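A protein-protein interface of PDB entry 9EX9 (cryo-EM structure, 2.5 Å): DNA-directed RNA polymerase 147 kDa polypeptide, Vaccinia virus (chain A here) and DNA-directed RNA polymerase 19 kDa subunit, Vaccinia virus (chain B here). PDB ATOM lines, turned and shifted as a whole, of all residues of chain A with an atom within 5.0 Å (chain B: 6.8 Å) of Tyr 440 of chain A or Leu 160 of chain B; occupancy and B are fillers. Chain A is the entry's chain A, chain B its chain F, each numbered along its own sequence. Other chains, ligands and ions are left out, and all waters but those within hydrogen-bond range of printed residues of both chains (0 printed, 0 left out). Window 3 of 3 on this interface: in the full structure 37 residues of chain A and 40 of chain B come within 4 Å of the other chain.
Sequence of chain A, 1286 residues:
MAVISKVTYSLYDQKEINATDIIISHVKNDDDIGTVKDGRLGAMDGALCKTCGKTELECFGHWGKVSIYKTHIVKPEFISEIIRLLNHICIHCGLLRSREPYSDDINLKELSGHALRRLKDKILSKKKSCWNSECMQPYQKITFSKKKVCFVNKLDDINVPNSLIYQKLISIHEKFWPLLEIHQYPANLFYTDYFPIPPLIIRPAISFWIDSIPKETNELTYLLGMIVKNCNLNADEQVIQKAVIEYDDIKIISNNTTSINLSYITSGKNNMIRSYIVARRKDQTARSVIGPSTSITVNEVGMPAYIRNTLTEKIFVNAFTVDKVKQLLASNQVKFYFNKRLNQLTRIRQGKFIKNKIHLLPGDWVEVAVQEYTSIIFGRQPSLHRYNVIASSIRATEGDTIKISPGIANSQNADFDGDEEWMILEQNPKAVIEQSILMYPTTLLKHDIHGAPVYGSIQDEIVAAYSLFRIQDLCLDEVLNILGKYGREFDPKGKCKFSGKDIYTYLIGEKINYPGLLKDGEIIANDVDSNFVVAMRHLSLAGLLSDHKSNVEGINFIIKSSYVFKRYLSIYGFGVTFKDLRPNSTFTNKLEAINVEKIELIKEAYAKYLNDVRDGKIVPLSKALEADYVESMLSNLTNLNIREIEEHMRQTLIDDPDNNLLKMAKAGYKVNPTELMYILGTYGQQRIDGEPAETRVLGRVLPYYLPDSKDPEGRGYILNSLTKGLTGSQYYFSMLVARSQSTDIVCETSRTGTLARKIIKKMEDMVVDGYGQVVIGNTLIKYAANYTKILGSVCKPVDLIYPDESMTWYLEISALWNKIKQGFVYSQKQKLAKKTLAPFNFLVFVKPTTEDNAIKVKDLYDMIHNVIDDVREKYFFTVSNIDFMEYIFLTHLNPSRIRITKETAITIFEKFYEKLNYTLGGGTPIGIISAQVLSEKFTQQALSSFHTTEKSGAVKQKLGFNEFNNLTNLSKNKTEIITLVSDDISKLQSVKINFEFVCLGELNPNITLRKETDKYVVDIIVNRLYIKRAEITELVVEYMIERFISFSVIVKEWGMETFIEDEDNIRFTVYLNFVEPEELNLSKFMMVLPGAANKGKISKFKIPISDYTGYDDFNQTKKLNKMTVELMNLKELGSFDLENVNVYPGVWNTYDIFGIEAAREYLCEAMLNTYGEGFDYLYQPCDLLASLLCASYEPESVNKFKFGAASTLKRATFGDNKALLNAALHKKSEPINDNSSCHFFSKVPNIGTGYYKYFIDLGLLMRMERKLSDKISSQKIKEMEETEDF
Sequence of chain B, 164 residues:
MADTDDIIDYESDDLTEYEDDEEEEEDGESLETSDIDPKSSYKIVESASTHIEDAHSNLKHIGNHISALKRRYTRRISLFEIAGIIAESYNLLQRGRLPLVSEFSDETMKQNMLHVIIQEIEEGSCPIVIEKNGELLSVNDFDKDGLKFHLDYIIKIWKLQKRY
The side-chain hydroxyl of Thr 443 of chain A lies within hydrogen-bond range of the side-chain hydroxyl of Tyr 153 of chain B (3.0 Å). OH of Tyr 153 of chain B is in hydrogen-bond range of O of Thr 442 of chain A, 3.5 Å away. The side-chain amino group (NZ) of Lys 162 of chain B is in hydrogen-bond range of the side-chain hydroxyl (OH) of Tyr 373 of chain A (3.4 Å). NE1 of Trp 158 of chain B is in hydrogen-bond range of OG of Ser 436 of chain A, 3.5 Å away. The side-chain amide nitrogen (NE2) of Gln 161 of chain B is in hydrogen-bond range of the backbone carbonyl oxygen (O) of Ser 436 of chain A (3.0 Å).
The side-chain amide oxygen of Gln 161 of chain B sits at hydrogen-bond distance from the guanidinium group of Arg 163 of chain B (2.7 Å). The backbone carbonyl oxygen (O) of Trp 158 of chain B is in hydrogen-bond range of the backbone NH (N) of Arg 163 of chain B, at 3.2 Å. O of Ile 437 of chain A lies within hydrogen-bond range of OG1 of Thr 443 of chain A (3.0 Å). The side-chain hydroxyl (OG1) of Thr 442 of chain A lies within hydrogen-bond range of the side-chain amide nitrogen (ND2) of Asn 299 of chain A, at 2.7 Å.
Among the printed residues, pairs that only touch across the chains: Tyr 440 of chain A with Gln 161 of chain B (3.4 Å), Ser 436 of chain A with Arg 163 of chain B (3.5 Å), Tyr 373 of chain A with Gln 161 of chain B (3.7 Å), Tyr 440 of chain A with Leu 160 of chain B (3.9 Å) and Ser 436 of chain A with Ile 157 of chain B (3.95 Å).
Of the printed residues of chain B, Tyr 373 of chain A touches Gln 161 and Lys 162. Tyr 440 of chain A touches just these residues of chain B: Leu 160 and Gln 161. Of the printed residues of chain B, Thr 442 of chain A touches Tyr 153 (3.5 Å). Leu 160 of chain B touches just one residue of chain A: Tyr 440. Of the printed residues of chain A, Gln 161 of chain B touches Tyr 373, Ser 436 and Tyr 440. The nearest printed residue of chain B that does not touch Ser 436 of chain A is Tyr 153 of chain B (7.3 Å).
Of the 11 printed residues of chain B, 7 touch a printed residue of chain A. Printed residues of chain B that touch a printed residue of chain A: Tyr 153, Ile 157, Trp 158, Leu 160, Gln 161, Lys 162 and Arg 163. Hydrophobic or aromatic side chains of chain B within 4 Å of the printed part of chain A: Tyr 153, Ile 157, Trp 158 and Leu 160. Printed residues of chain A that touch a printed residue of chain B: Tyr 373, Ser 436, Tyr 440, Thr 442 and Thr 443. Hydrophobic or aromatic side chains of chain A within 4 Å of the printed part of chain B: Tyr 373 and Tyr 440. Among the printed residues, no Asp or Glu carboxylate lies within 4 Å of a Lys or Arg side-chain nitrogen of the other chain.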
ATOM      1  N   ASN A 299      17.612   3.150  26.027  1.00  0.00           N
ATOM      2  CA  ASN A 299      17.778   4.177  27.046  1.00  0.00           C
ATOM      3  C   ASN A 299      17.939   3.616  28.452  1.00  0.00           C
ATOM      4  O   ASN A 299      18.260   4.379  29.366  1.00  0.00           O
ATOM      5  CB  ASN A 299      16.581   5.131  27.039  1.00  0.00           C
ATOM      6  CG  ASN A 299      16.472   5.928  25.763  1.00  0.00           C
ATOM      7  OD1 ASN A 299      15.426   5.947  25.123  1.00  0.00           O
ATOM      8  ND2 ASN A 299      17.546   6.604  25.391  1.00  0.00           N
ATOM      9  N   TYR A 373      14.777   4.167  37.656  1.00  0.00           N
ATOM     10  CA  TYR A 373      14.864   5.345  36.800  1.00  0.00           C
ATOM     11  C   TYR A 373      15.900   6.346  37.286  1.00  0.00           C
ATOM     12  O   TYR A 373      15.919   7.484  36.811  1.00  0.00           O
ATOM     13  CB  TYR A 373      13.506   6.030  36.636  1.00  0.00           C
ATOM     14  CG  TYR A 373      12.574   5.251  35.745  1.00  0.00           C
ATOM     15  CD1 TYR A 373      12.685   5.322  34.367  1.00  0.00           C
ATOM     16  CD2 TYR A 373      11.599   4.429  36.280  1.00  0.00           C
ATOM     17  CE1 TYR A 373      11.847   4.607  33.551  1.00  0.00           C
ATOM     18  CE2 TYR A 373      10.753   3.714  35.469  1.00  0.00           C
ATOM     19  CZ  TYR A 373      10.883   3.806  34.106  1.00  0.00           C
ATOM     20  OH  TYR A 373      10.044   3.092  33.290  1.00  0.00           O
ATOM     21  N   ALA A 391      25.354   6.827  30.372  1.00  0.00           N
ATOM     22  CA  ALA A 391      24.510   6.934  31.556  1.00  0.00           C
ATOM     23  C   ALA A 391      23.073   6.610  31.178  1.00  0.00           C
ATOM     24  O   ALA A 391      22.489   7.281  30.325  1.00  0.00           O
ATOM     25  CB  ALA A 391      24.596   8.334  32.160  1.00  0.00           C
ATOM     26  N   SER A 393      19.020   4.741  32.463  1.00  0.00           N
ATOM     27  CA  SER A 393      18.050   4.614  33.541  1.00  0.00           C
ATOM     28  C   SER A 393      18.009   3.189  34.073  1.00  0.00           C
ATOM     29  O   SER A 393      18.059   2.223  33.310  1.00  0.00           O
ATOM     30  CB  SER A 393      16.660   5.015  33.052  1.00  0.00           C
ATOM     31  OG  SER A 393      16.658   6.338  32.552  1.00  0.00           O
ATOM     32  N   GLN A 435      24.487  14.021  33.466  1.00  0.00           N
ATOM     33  CA  GLN A 435      24.191  12.660  33.037  1.00  0.00           C
ATOM     34  C   GLN A 435      22.844  12.592  32.338  1.00  0.00           C
ATOM     35  O   GLN A 435      22.693  11.889  31.335  1.00  0.00           O
ATOM     36  CB  GLN A 435      24.196  11.711  34.230  1.00  0.00           C
ATOM     37  CG  GLN A 435      25.544  11.493  34.867  1.00  0.00           C
ATOM     38  CD  GLN A 435      25.434  10.763  36.184  1.00  0.00           C
ATOM     39  OE1 GLN A 435      24.830   9.699  36.267  1.00  0.00           O
ATOM     40  NE2 GLN A 435      26.001  11.341  37.228  1.00  0.00           N
ATOM     41  N   SER A 436      21.847  13.299  32.867  1.00  0.00           N
ATOM     42  CA  SER A 436      20.516  13.221  32.283  1.00  0.00           C
ATOM     43  C   SER A 436      20.477  13.821  30.888  1.00  0.00           C
ATOM     44  O   SER A 436      19.720  13.346  30.037  1.00  0.00           O
ATOM     45  CB  SER A 436      19.506  13.924  33.182  1.00  0.00           C
ATOM     46  OG  SER A 436      19.786  15.307  33.267  1.00  0.00           O
ATOM     47  N   ILE A 437      21.272  14.856  30.627  1.00  0.00           N
ATOM     48  CA  ILE A 437      21.212  15.520  29.329  1.00  0.00           C
ATOM     49  C   ILE A 437      22.314  15.032  28.394  1.00  0.00           C
ATOM     50  O   ILE A 437      22.032  14.499  27.317  1.00  0.00           O
ATOM     51  CB  ILE A 437      21.285  17.047  29.488  1.00  0.00           C
ATOM     52  CG1 ILE A 437      20.058  17.563  30.237  1.00  0.00           C
ATOM     53  CG2 ILE A 437      21.387  17.704  28.128  1.00  0.00           C
ATOM     54  CD1 ILE A 437      20.172  18.999  30.685  1.00  0.00           C
ATOM     55  N   LEU A 438      23.576  15.214  28.789  1.00  0.00           N
ATOM     56  CA  LEU A 438      24.680  15.067  27.842  1.00  0.00           C
ATOM     57  C   LEU A 438      25.012  13.610  27.539  1.00  0.00           C
ATOM     58  O   LEU A 438      25.364  13.281  26.401  1.00  0.00           O
ATOM     59  CB  LEU A 438      25.920  15.778  28.377  1.00  0.00           C
ATOM     60  CG  LEU A 438      25.797  17.288  28.552  1.00  0.00           C
ATOM     61  CD1 LEU A 438      27.043  17.837  29.201  1.00  0.00           C
ATOM     62  CD2 LEU A 438      25.552  17.973  27.226  1.00  0.00           C
ATOM     63  N   MET A 439      24.929  12.728  28.527  1.00  0.00           N
ATOM     64  CA  MET A 439      25.338  11.340  28.363  1.00  0.00           C
ATOM     65  C   MET A 439      24.166  10.412  28.090  1.00  0.00           C
ATOM     66  O   MET A 439      24.333   9.193  28.137  1.00  0.00           O
ATOM     67  CB  MET A 439      26.096  10.869  29.602  1.00  0.00           C
ATOM     68  CG  MET A 439      27.357  11.660  29.885  1.00  0.00           C
ATOM     69  SD  MET A 439      28.191  11.164  31.394  1.00  0.00           S
ATOM     70  CE  MET A 439      28.457   9.428  31.071  1.00  0.00           C
ATOM     71  N   TYR A 440      22.991  10.961  27.816  1.00  0.00           N
ATOM     72  CA  TYR A 440      21.825  10.140  27.541  1.00  0.00           C
ATOM     73  C   TYR A 440      21.951   9.503  26.159  1.00  0.00           C
ATOM     74  O   TYR A 440      22.303  10.187  25.196  1.00  0.00           O
ATOM     75  CB  TYR A 440      20.566  10.999  27.616  1.00  0.00           C
ATOM     76  CG  TYR A 440      19.273  10.243  27.779  1.00  0.00           C
ATOM     77  CD1 TYR A 440      19.097   9.337  28.810  1.00  0.00           C
ATOM     78  CD2 TYR A 440      18.212  10.466  26.919  1.00  0.00           C
ATOM     79  CE1 TYR A 440      17.910   8.658  28.962  1.00  0.00           C
ATOM     80  CE2 TYR A 440      17.026   9.792  27.064  1.00  0.00           C
ATOM     81  CZ  TYR A 440      16.880   8.893  28.088  1.00  0.00           C
ATOM     82  OH  TYR A 440      15.695   8.223  28.232  1.00  0.00           O
ATOM     83  N   PRO A 441      21.663   8.208  26.020  1.00  0.00           N
ATOM     84  CA  PRO A 441      21.809   7.580  24.699  1.00  0.00           C
ATOM     85  C   PRO A 441      21.046   8.292  23.597  1.00  0.00           C
ATOM     86  O   PRO A 441      21.533   8.365  22.465  1.00  0.00           O
ATOM     87  CB  PRO A 441      21.276   6.165  24.937  1.00  0.00           C
ATOM     88  CG  PRO A 441      21.516   5.915  26.360  1.00  0.00           C
ATOM     89  CD  PRO A 441      21.300   7.219  27.047  1.00  0.00           C
ATOM     90  N   THR A 442      19.864   8.825  23.897  1.00  0.00           N
ATOM     91  CA  THR A 442      19.093   9.517  22.872  1.00  0.00           C
ATOM     92  C   THR A 442      19.843  10.720  22.317  1.00  0.00           C
ATOM     93  O   THR A 442      19.548  11.173  21.209  1.00  0.00           O
ATOM     94  CB  THR A 442      17.749   9.960  23.438  1.00  0.00           C
ATOM     95  OG1 THR A 442      17.053   8.822  23.954  1.00  0.00           O
ATOM     96  CG2 THR A 442      16.914  10.617  22.365  1.00  0.00           C
ATOM     97  N   THR A 443      20.801  11.259  23.071  1.00  0.00           N
ATOM     98  CA  THR A 443      21.582  12.390  22.593  1.00  0.00           C
ATOM     99  C   THR A 443      22.781  11.965  21.758  1.00  0.00           C
ATOM    100  O   THR A 443      23.356  12.800  21.056  1.00  0.00           O
ATOM    101  CB  THR A 443      22.060  13.231  23.779  1.00  0.00           C
ATOM    102  OG1 THR A 443      20.956  13.514  24.641  1.00  0.00           O
ATOM    103  CG2 THR A 443      22.665  14.537  23.307  1.00  0.00           C
ATOM    104  N   LEU A 444      23.163  10.688  21.809  1.00  0.00           N
ATOM    105  CA  LEU A 444      24.339  10.180  21.120  1.00  0.00           C
ATOM    106  C   LEU A 444      23.985   9.399  19.863  1.00  0.00           C
ATOM    107  O   LEU A 444      24.782   8.571  19.415  1.00  0.00           O
ATOM    108  CB  LEU A 444      25.149   9.291  22.059  1.00  0.00           C
ATOM    109  CG  LEU A 444      25.455   9.835  23.449  1.00  0.00           C
ATOM    110  CD1 LEU A 444      25.981   8.727  24.325  1.00  0.00           C
ATOM    111  CD2 LEU A 444      26.449  10.964  23.369  1.00  0.00           C
ATOM    112  N   TYR B 153      13.652  20.060  23.548  1.00  0.00           N
ATOM    113  CA  TYR B 153      14.356  18.780  23.507  1.00  0.00           C
ATOM    114  C   TYR B 153      14.581  18.234  24.915  1.00  0.00           C
ATOM    115  O   TYR B 153      14.317  17.052  25.197  1.00  0.00           O
ATOM    116  CB  TYR B 153      15.686  18.932  22.772  1.00  0.00           C
ATOM    117  CG  TYR B 153      16.501  17.667  22.771  1.00  0.00           C
ATOM    118  CD1 TYR B 153      16.149  16.598  21.965  1.00  0.00           C
ATOM    119  CD2 TYR B 153      17.618  17.535  23.579  1.00  0.00           C
ATOM    120  CE1 TYR B 153      16.884  15.433  21.966  1.00  0.00           C
ATOM    121  CE2 TYR B 153      18.355  16.376  23.588  1.00  0.00           C
ATOM    122  CZ  TYR B 153      17.987  15.330  22.777  1.00  0.00           C
ATOM    123  OH  TYR B 153      18.726  14.176  22.780  1.00  0.00           O
ATOM    124  N   ILE B 155      13.074  18.822  27.767  1.00  0.00           N
ATOM    125  CA  ILE B 155      11.877  18.403  28.481  1.00  0.00           C
ATOM    126  C   ILE B 155      11.355  17.089  27.923  1.00  0.00           C
ATOM    127  O   ILE B 155      10.883  16.232  28.676  1.00  0.00           O
ATOM    128  CB  ILE B 155      10.816  19.515  28.438  1.00  0.00           C
ATOM    129  CG1 ILE B 155      11.303  20.714  29.253  1.00  0.00           C
ATOM    130  CG2 ILE B 155       9.498  19.000  28.978  1.00  0.00           C
ATOM    131  CD1 ILE B 155      10.450  21.938  29.128  1.00  0.00           C
ATOM    132  N   LYS B 156      11.431  16.892  26.605  1.00  0.00           N
ATOM    133  CA  LYS B 156      11.046  15.591  26.061  1.00  0.00           C
ATOM    134  C   LYS B 156      11.863  14.474  26.695  1.00  0.00           C
ATOM    135  O   LYS B 156      11.310  13.503  27.237  1.00  0.00           O
ATOM    136  CB  LYS B 156      11.229  15.569  24.545  1.00  0.00           C
ATOM    137  CG  LYS B 156      10.126  16.227  23.760  1.00  0.00           C
ATOM    138  CD  LYS B 156      10.451  16.203  22.287  1.00  0.00           C
ATOM    139  CE  LYS B 156       9.496  17.062  21.495  1.00  0.00           C
ATOM    140  NZ  LYS B 156       9.932  17.208  20.083  1.00  0.00           N
ATOM    141  N   ILE B 157      13.190  14.601  26.658  1.00  0.00           N
ATOM    142  CA  ILE B 157      14.001  13.490  27.149  1.00  0.00           C
ATOM    143  C   ILE B 157      13.814  13.311  28.652  1.00  0.00           C
ATOM    144  O   ILE B 157      13.859  12.184  29.151  1.00  0.00           O
ATOM    145  CB  ILE B 157      15.482  13.666  26.770  1.00  0.00           C
ATOM    146  CG1 ILE B 157      16.073  14.925  27.390  1.00  0.00           C
ATOM    147  CG2 ILE B 157      15.624  13.706  25.266  1.00  0.00           C
ATOM    148  CD1 ILE B 157      17.556  15.036  27.195  1.00  0.00           C
ATOM    149  N   TRP B 158      13.593  14.397  29.397  1.00  0.00           N
ATOM    150  CA  TRP B 158      13.287  14.261  30.819  1.00  0.00           C
ATOM    151  C   TRP B 158      11.999  13.484  31.035  1.00  0.00           C
ATOM    152  O   TRP B 158      11.924  12.629  31.923  1.00  0.00           O
ATOM    153  CB  TRP B 158      13.178  15.635  31.473  1.00  0.00           C
ATOM    154  CG  TRP B 158      14.468  16.221  31.926  1.00  0.00           C
ATOM    155  CD1 TRP B 158      15.674  15.595  32.007  1.00  0.00           C
ATOM    156  CD2 TRP B 158      14.682  17.562  32.366  1.00  0.00           C
ATOM    157  NE1 TRP B 158      16.626  16.463  32.470  1.00  0.00           N
ATOM    158  CE2 TRP B 158      16.041  17.678  32.699  1.00  0.00           C
ATOM    159  CE3 TRP B 158      13.855  18.676  32.511  1.00  0.00           C
ATOM    160  CZ2 TRP B 158      16.592  18.864  33.165  1.00  0.00           C
ATOM    161  CZ3 TRP B 158      14.402  19.847  32.972  1.00  0.00           C
ATOM    162  CH2 TRP B 158      15.756  19.935  33.296  1.00  0.00           C
ATOM    163  N   LYS B 159      10.966  13.773  30.244  1.00  0.00           N
ATOM    164  CA  LYS B 159       9.722  13.028  30.376  1.00  0.00           C
ATOM    165  C   LYS B 159       9.953  11.549  30.122  1.00  0.00           C
ATOM    166  O   LYS B 159       9.339  10.698  30.772  1.00  0.00           O
ATOM    167  CB  LYS B 159       8.669  13.578  29.420  1.00  0.00           C
ATOM    168  CG  LYS B 159       7.967  14.808  29.943  1.00  0.00           C
ATOM    169  CD  LYS B 159       6.932  15.322  28.968  1.00  0.00           C
ATOM    170  CE  LYS B 159       6.217  16.536  29.523  1.00  0.00           C
ATOM    171  NZ  LYS B 159       5.214  17.078  28.574  1.00  0.00           N
ATOM    172  N   LEU B 160      10.840  11.220  29.182  1.00  0.00           N
ATOM    173  CA  LEU B 160      11.171   9.811  28.984  1.00  0.00           C
ATOM    174  C   LEU B 160      11.792   9.195  30.231  1.00  0.00           C
ATOM    175  O   LEU B 160      11.614   7.999  30.481  1.00  0.00           O
ATOM    176  CB  LEU B 160      12.122   9.644  27.801  1.00  0.00           C
ATOM    177  CG  LEU B 160      11.516   9.705  26.404  1.00  0.00           C
ATOM    178  CD1 LEU B 160      12.600   9.556  25.357  1.00  0.00           C
ATOM    179  CD2 LEU B 160      10.469   8.631  26.233  1.00  0.00           C
ATOM    180  N   GLN B 161      12.520   9.980  31.021  1.00  0.00           N
ATOM    181  CA  GLN B 161      13.234   9.469  32.184  1.00  0.00           C
ATOM    182  C   GLN B 161      12.397   9.471  33.455  1.00  0.00           C
ATOM    183  O   GLN B 161      12.866   8.975  34.482  1.00  0.00           O
ATOM    184  CB  GLN B 161      14.499  10.292  32.431  1.00  0.00           C
ATOM    185  CG  GLN B 161      15.485  10.283  31.295  1.00  0.00           C
ATOM    186  CD  GLN B 161      16.526  11.354  31.445  1.00  0.00           C
ATOM    187  OE1 GLN B 161      16.718  11.890  32.528  1.00  0.00           O
ATOM    188  NE2 GLN B 161      17.196  11.686  30.358  1.00  0.00           N
ATOM    189  N   LYS B 162      11.185  10.024  33.415  1.00  0.00           N
ATOM    190  CA  LYS B 162      10.319  10.145  34.584  1.00  0.00           C
ATOM    191  C   LYS B 162      10.804  11.220  35.551  1.00  0.00           C
ATOM    192  O   LYS B 162      10.606  11.104  36.760  1.00  0.00           O
ATOM    193  CB  LYS B 162      10.176   8.810  35.320  1.00  0.00           C
ATOM    194  CG  LYS B 162       9.727   7.660  34.449  1.00  0.00           C
ATOM    195  CD  LYS B 162       8.368   7.927  33.849  1.00  0.00           C
ATOM    196  CE  LYS B 162       7.700   6.644  33.394  1.00  0.00           C
ATOM    197  NZ  LYS B 162       8.473   5.950  32.334  1.00  0.00           N
ATOM    198  N   ARG B 163      11.443  12.270  35.042  1.00  0.00           N
ATOM    199  CA  ARG B 163      11.873  13.386  35.875  1.00  0.00           C
ATOM    200  C   ARG B 163      10.911  14.559  35.853  1.00  0.00           C
ATOM    201  O   ARG B 163      10.843  15.306  36.833  1.00  0.00           O
ATOM    202  CB  ARG B 163      13.243  13.901  35.427  1.00  0.00           C
ATOM    203  CG  ARG B 163      14.385  12.955  35.634  1.00  0.00           C
ATOM    204  CD  ARG B 163      15.693  13.649  35.332  1.00  0.00           C
ATOM    205  NE  ARG B 163      16.762  12.700  35.052  1.00  0.00           N
ATOM    206  CZ  ARG B 163      17.453  12.055  35.978  1.00  0.00           C
ATOM    207  NH1 ARG B 163      17.205  12.219  37.265  1.00  0.00           N
ATOM    208  NH2 ARG B 163      18.412  11.217  35.603  1.00  0.00           N
ATOM    209  N   TYR B 164      10.186  14.752  34.760  1.00  0.00           N
ATOM    210  CA  TYR B 164       9.387  15.950  34.576  1.00  0.00           C
ATOM    211  C   TYR B 164       7.905  15.613  34.606  1.00  0.00           C
ATOM    212  O   TYR B 164       7.498  14.537  34.170  1.00  0.00           O
ATOM    213  CB  TYR B 164       9.752  16.623  33.254  1.00  0.00           C
ATOM    214  CG  TYR B 164       9.395  18.086  33.185  1.00  0.00           C
ATOM    215  CD1 TYR B 164      10.147  19.032  33.859  1.00  0.00           C
ATOM    216  CD2 TYR B 164       8.317  18.522  32.437  1.00  0.00           C
ATOM    217  CE1 TYR B 164       9.832  20.366  33.797  1.00  0.00           C
ATOM    218  CE2 TYR B 164       7.994  19.856  32.370  1.00  0.00           C
ATOM    219  CZ  TYR B 164       8.756  20.773  33.050  1.00  0.00           C
ATOM    220  OH  TYR B 164       8.436  22.106  32.986  1.00  0.00           O
